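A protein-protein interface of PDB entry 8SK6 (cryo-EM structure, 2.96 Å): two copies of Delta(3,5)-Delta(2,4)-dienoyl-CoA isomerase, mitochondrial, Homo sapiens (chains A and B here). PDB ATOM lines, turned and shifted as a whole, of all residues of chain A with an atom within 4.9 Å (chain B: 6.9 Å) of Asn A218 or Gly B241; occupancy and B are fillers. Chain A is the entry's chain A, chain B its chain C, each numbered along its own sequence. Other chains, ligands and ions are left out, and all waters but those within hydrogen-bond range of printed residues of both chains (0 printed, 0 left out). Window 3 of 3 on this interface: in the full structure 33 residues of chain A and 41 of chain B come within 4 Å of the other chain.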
ATOM      1  N   ILE A 216      22.867  16.795 -18.241  1.00  0.00           N
ATOM      2  CA  ILE A 216      22.082  17.953 -17.836  1.00  0.00           C
ATOM      3  C   ILE A 216      21.861  18.839 -19.052  1.00  0.00           C
ATOM      4  O   ILE A 216      22.617  18.802 -20.024  1.00  0.00           O
ATOM      5  CB  ILE A 216      22.748  18.756 -16.697  1.00  0.00           C
ATOM      6  CG1 ILE A 216      24.179  19.140 -17.069  1.00  0.00           C
ATOM      7  CG2 ILE A 216      22.736  17.960 -15.409  1.00  0.00           C
ATOM      8  CD1 ILE A 216      24.923  19.823 -15.946  1.00  0.00           C
ATOM      9  N   GLY A 217      20.803  19.643 -18.988  1.00  0.00           N
ATOM     10  CA  GLY A 217      20.426  20.475 -20.113  1.00  0.00           C
ATOM     11  C   GLY A 217      20.952  21.894 -20.043  1.00  0.00           C
ATOM     12  O   GLY A 217      21.023  22.583 -21.064  1.00  0.00           O
ATOM     13  N   ASN A 218      21.329  22.344 -18.847  1.00  0.00           N
ATOM     14  CA  ASN A 218      21.816  23.708 -18.650  1.00  0.00           C
ATOM     15  C   ASN A 218      23.260  23.779 -19.138  1.00  0.00           C
ATOM     16  O   ASN A 218      24.221  23.726 -18.366  1.00  0.00           O
ATOM     17  CB  ASN A 218      21.687  24.118 -17.189  1.00  0.00           C
ATOM     18  CG  ASN A 218      21.966  25.591 -16.970  1.00  0.00           C
ATOM     19  OD1 ASN A 218      22.120  26.352 -17.922  1.00  0.00           O
ATOM     20  ND2 ASN A 218      22.024  26.000 -15.709  1.00  0.00           N
ATOM     21  N   GLN A 219      23.408  23.898 -20.461  1.00  0.00           N
ATOM     22  CA  GLN A 219      24.740  23.924 -21.057  1.00  0.00           C
ATOM     23  C   GLN A 219      25.516  25.170 -20.659  1.00  0.00           C
ATOM     24  O   GLN A 219      26.752  25.157 -20.670  1.00  0.00           O
ATOM     25  CB  GLN A 219      24.638  23.828 -22.577  1.00  0.00           C
ATOM     26  CG  GLN A 219      24.050  22.523 -23.067  1.00  0.00           C
ATOM     27  CD  GLN A 219      24.876  21.326 -22.655  1.00  0.00           C
ATOM     28  OE1 GLN A 219      26.101  21.400 -22.578  1.00  0.00           O
ATOM     29  NE2 GLN A 219      24.207  20.211 -22.385  1.00  0.00           N
ATOM     30  N   SER A 220      24.819  26.254 -20.318  1.00  0.00           N
ATOM     31  CA  SER A 220      25.508  27.446 -19.839  1.00  0.00           C
ATOM     32  C   SER A 220      26.238  27.165 -18.533  1.00  0.00           C
ATOM     33  O   SER A 220      27.355  27.647 -18.319  1.00  0.00           O
ATOM     34  CB  SER A 220      24.517  28.594 -19.664  1.00  0.00           C
ATOM     35  OG  SER A 220      25.165  29.747 -19.161  1.00  0.00           O
ATOM     36  N   LEU A 221      25.616  26.390 -17.643  1.00  0.00           N
ATOM     37  CA  LEU A 221      26.270  26.027 -16.391  1.00  0.00           C
ATOM     38  C   LEU A 221      27.459  25.106 -16.631  1.00  0.00           C
ATOM     39  O   LEU A 221      28.483  25.218 -15.947  1.00  0.00           O
ATOM     40  CB  LEU A 221      25.266  25.371 -15.445  1.00  0.00           C
ATOM     41  CG  LEU A 221      25.804  25.024 -14.059  1.00  0.00           C
ATOM     42  CD1 LEU A 221      26.364  26.263 -13.391  1.00  0.00           C
ATOM     43  CD2 LEU A 221      24.720  24.403 -13.207  1.00  0.00           C
ATOM     44  N   VAL A 222      27.342  24.188 -17.593  1.00  0.00           N
ATOM     45  CA  VAL A 222      28.423  23.241 -17.861  1.00  0.00           C
ATOM     46  C   VAL A 222      29.689  23.984 -18.268  1.00  0.00           C
ATOM     47  O   VAL A 222      30.788  23.687 -17.787  1.00  0.00           O
ATOM     48  CB  VAL A 222      27.998  22.229 -18.937  1.00  0.00           C
ATOM     49  CG1 VAL A 222      29.096  21.207 -19.166  1.00  0.00           C
ATOM     50  CG2 VAL A 222      26.707  21.547 -18.539  1.00  0.00           C
ATOM     51  N   ARG B 185      25.969  32.500 -20.884  1.00  0.00           N
ATOM     52  CA  ARG B 185      24.979  33.544 -21.100  1.00  0.00           C
ATOM     53  C   ARG B 185      24.561  34.142 -19.765  1.00  0.00           C
ATOM     54  O   ARG B 185      24.120  33.420 -18.866  1.00  0.00           O
ATOM     55  CB  ARG B 185      23.759  32.994 -21.839  1.00  0.00           C
ATOM     56  CG  ARG B 185      24.013  32.709 -23.305  1.00  0.00           C
ATOM     57  CD  ARG B 185      22.965  31.777 -23.874  1.00  0.00           C
ATOM     58  NE  ARG B 185      23.093  30.432 -23.327  1.00  0.00           N
ATOM     59  CZ  ARG B 185      23.899  29.500 -23.818  1.00  0.00           C
ATOM     60  NH1 ARG B 185      24.662  29.734 -24.872  1.00  0.00           N
ATOM     61  NH2 ARG B 185      23.939  28.306 -23.236  1.00  0.00           N
ATOM     62  N   VAL B 215      21.080  23.861 -26.181  1.00  0.00           N
ATOM     63  CA  VAL B 215      21.613  24.565 -25.020  1.00  0.00           C
ATOM     64  C   VAL B 215      20.671  24.519 -23.821  1.00  0.00           C
ATOM     65  O   VAL B 215      21.080  24.905 -22.715  1.00  0.00           O
ATOM     66  CB  VAL B 215      21.960  26.028 -25.361  1.00  0.00           C
ATOM     67  CG1 VAL B 215      23.018  26.081 -26.446  1.00  0.00           C
ATOM     68  CG2 VAL B 215      20.714  26.786 -25.778  1.00  0.00           C
ATOM     69  N   ILE B 216      19.426  24.076 -24.004  1.00  0.00           N
ATOM     70  CA  ILE B 216      18.495  23.875 -22.903  1.00  0.00           C
ATOM     71  C   ILE B 216      17.801  22.533 -23.093  1.00  0.00           C
ATOM     72  O   ILE B 216      17.706  22.007 -24.203  1.00  0.00           O
ATOM     73  CB  ILE B 216      17.454  25.010 -22.790  1.00  0.00           C
ATOM     74  CG1 ILE B 216      16.732  25.220 -24.118  1.00  0.00           C
ATOM     75  CG2 ILE B 216      18.119  26.297 -22.345  1.00  0.00           C
ATOM     76  CD1 ILE B 216      15.794  26.405 -24.106  1.00  0.00           C
ATOM     77  N   GLY B 217      17.314  21.981 -21.986  1.00  0.00           N
ATOM     78  CA  GLY B 217      16.709  20.665 -22.009  1.00  0.00           C
ATOM     79  C   GLY B 217      15.201  20.672 -22.133  1.00  0.00           C
ATOM     80  O   GLY B 217      14.602  19.669 -22.527  1.00  0.00           O
ATOM     81  N   GLU B 236      11.986  33.588 -16.330  1.00  0.00           N
ATOM     82  CA  GLU B 236      11.668  32.342 -17.018  1.00  0.00           C
ATOM     83  C   GLU B 236      12.896  31.772 -17.717  1.00  0.00           C
ATOM     84  O   GLU B 236      13.066  30.549 -17.791  1.00  0.00           O
ATOM     85  CB  GLU B 236      10.536  32.571 -18.019  1.00  0.00           C
ATOM     86  CG  GLU B 236      10.072  31.313 -18.730  1.00  0.00           C
ATOM     87  CD  GLU B 236       8.938  31.580 -19.699  1.00  0.00           C
ATOM     88  OE1 GLU B 236       8.534  32.752 -19.839  1.00  0.00           O
ATOM     89  OE2 GLU B 236       8.450  30.614 -20.323  1.00  0.00           O
ATOM     90  N   ALA B 237      13.759  32.644 -18.243  1.00  0.00           N
ATOM     91  CA  ALA B 237      14.970  32.181 -18.914  1.00  0.00           C
ATOM     92  C   ALA B 237      15.894  31.452 -17.949  1.00  0.00           C
ATOM     93  O   ALA B 237      16.480  30.420 -18.299  1.00  0.00           O
ATOM     94  CB  ALA B 237      15.694  33.360 -19.562  1.00  0.00           C
ATOM     95  N   LEU B 238      16.045  31.976 -16.731  1.00  0.00           N
ATOM     96  CA  LEU B 238      16.899  31.325 -15.744  1.00  0.00           C
ATOM     97  C   LEU B 238      16.359  29.952 -15.364  1.00  0.00           C
ATOM     98  O   LEU B 238      17.127  28.997 -15.204  1.00  0.00           O
ATOM     99  CB  LEU B 238      17.038  32.208 -14.505  1.00  0.00           C
ATOM    100  CG  LEU B 238      17.880  31.639 -13.364  1.00  0.00           C
ATOM    101  CD1 LEU B 238      19.300  31.374 -13.829  1.00  0.00           C
ATOM    102  CD2 LEU B 238      17.871  32.575 -12.169  1.00  0.00           C
ATOM    103  N   GLY B 239      15.039  29.837 -15.214  1.00  0.00           N
ATOM    104  CA  GLY B 239      14.454  28.549 -14.876  1.00  0.00           C
ATOM    105  C   GLY B 239      14.662  27.509 -15.959  1.00  0.00           C
ATOM    106  O   GLY B 239      14.808  26.319 -15.670  1.00  0.00           O
ATOM    107  N   SER B 240      14.677  27.940 -17.221  1.00  0.00           N
ATOM    108  CA  SER B 240      14.861  27.021 -18.336  1.00  0.00           C
ATOM    109  C   SER B 240      16.325  26.743 -18.643  1.00  0.00           C
ATOM    110  O   SER B 240      16.610  25.877 -19.476  1.00  0.00           O
ATOM    111  CB  SER B 240      14.176  27.569 -19.586  1.00  0.00           C
ATOM    112  OG  SER B 240      14.718  28.824 -19.952  1.00  0.00           O
ATOM    113  N   GLY B 241      17.252  27.445 -18.000  1.00  0.00           N
ATOM    114  CA  GLY B 241      18.664  27.206 -18.206  1.00  0.00           C
ATOM    115  C   GLY B 241      19.280  27.900 -19.397  1.00  0.00           C
ATOM    116  O   GLY B 241      20.418  27.575 -19.758  1.00  0.00           O
ATOM    117  N   LEU B 242      18.571  28.837 -20.029  1.00  0.00           N
ATOM    118  CA  LEU B 242      19.173  29.584 -21.130  1.00  0.00           C
ATOM    119  C   LEU B 242      20.296  30.482 -20.632  1.00  0.00           C
ATOM    120  O   LEU B 242      21.321  30.635 -21.305  1.00  0.00           O
ATOM    121  CB  LEU B 242      18.111  30.405 -21.858  1.00  0.00           C
ATOM    122  CG  LEU B 242      18.609  31.132 -23.107  1.00  0.00           C
ATOM    123  CD1 LEU B 242      19.174  30.141 -24.109  1.00  0.00           C
ATOM    124  CD2 LEU B 242      17.502  31.955 -23.739  1.00  0.00           C
ATOM    125  N   VAL B 243      20.124  31.076 -19.456  1.00  0.00           N
ATOM    126  CA  VAL B 243      21.141  31.918 -18.842  1.00  0.00           C
ATOM    127  C   VAL B 243      21.638  31.232 -17.579  1.00  0.00           C
ATOM    128  O   VAL B 243      20.966  30.362 -17.014  1.00  0.00           O
ATOM    129  CB  VAL B 243      20.607  33.328 -18.522  1.00  0.00           C
ATOM    130  CG1 VAL B 243      20.031  33.972 -19.770  1.00  0.00           C
ATOM    131  CG2 VAL B 243      19.568  33.260 -17.422  1.00  0.00           C
ATOM    132  N   SER B 244      22.832  31.624 -17.142  1.00  0.00           N
ATOM    133  CA  SER B 244      23.423  31.046 -15.942  1.00  0.00           C
ATOM    134  C   SER B 244      23.108  31.857 -14.693  1.00  0.00           C
ATOM    135  O   SER B 244      22.918  31.284 -13.616  1.00  0.00           O
ATOM    136  CB  SER B 244      24.940  30.921 -16.111  1.00  0.00           C
ATOM    137  OG  SER B 244      25.533  30.368 -14.951  1.00  0.00           O
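O of Gly A217 touches CA of Ile B216, at 3.4 Å.
Gly B217 touches Gly A217 (N to O, 3.9 Å).
Ser A220 touches Ser B244 (OG to CB, 3.3 Å).
Of chain B, only Gly B241 comes within 4 Å of Asn A218.
Of the printed residues of chain B, Ser A220 touches Arg B185 (3.3 Å) and Ser B244 (3.3 Å).
Printed residues of chain A within 4 Å of Ile B216: Gly A217.
Gly B241 touches just one residue of chain A: Asn A218 (2.8 Å).
Val B243 touches none of the printed residues of chain A.
Of the printed residues of chain A, Ser B244 touches Ser A220.
The nearest printed residue of chain A that does not touch Ile B216 is Gln A219 (5.0 Å).
Of the 7 printed residues of chain A, 4 touch a printed residue of chain B.
Of the 13 printed residues of chain B, 6 touch a printed residue of chain A.
Among the printed residues, no Asp or Glu carboxylate lies within 4 Å of a Lys or Arg side-chain nitrogen of the other chain.
N of Gln A219 lies within hydrogen-bond range of O of Val B215, 3.4 Å away.
The side-chain hydroxyl of Ser A220 sits at hydrogen-bond distance from the backbone NH of Arg B185 (3.3 Å).
O of Gly A217 lies close to O of Val B215.
OD1 of Asn A218 sits close to O of Gly B241.
The backbone carbonyl oxygen (O) of Ile A216 sits at hydrogen-bond distance from the side-chain amide nitrogen (NE2) of Gln A219, 3.2 Å away.
NE of Arg B185 is in hydrogen-bond range of O of Leu B242, at 2.7 Å.
The backbone carbonyl oxygen (O) of Arg B185 is in hydrogen-bond range of the backbone NH (N) of Ser B244 (2.8 Å).
Gly A217 touches Ile B216, but with the chains exchanged Ile A216 does not touch Gly B217 (6.2 Å).
Gly A217 touches its own counterpart, Gly B217.
Positions printed for both chains: 216 and 217.
Of the 7 pairs that touch across the chains among the printed residues, 1 has its exchanged pair printed and touching as well.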
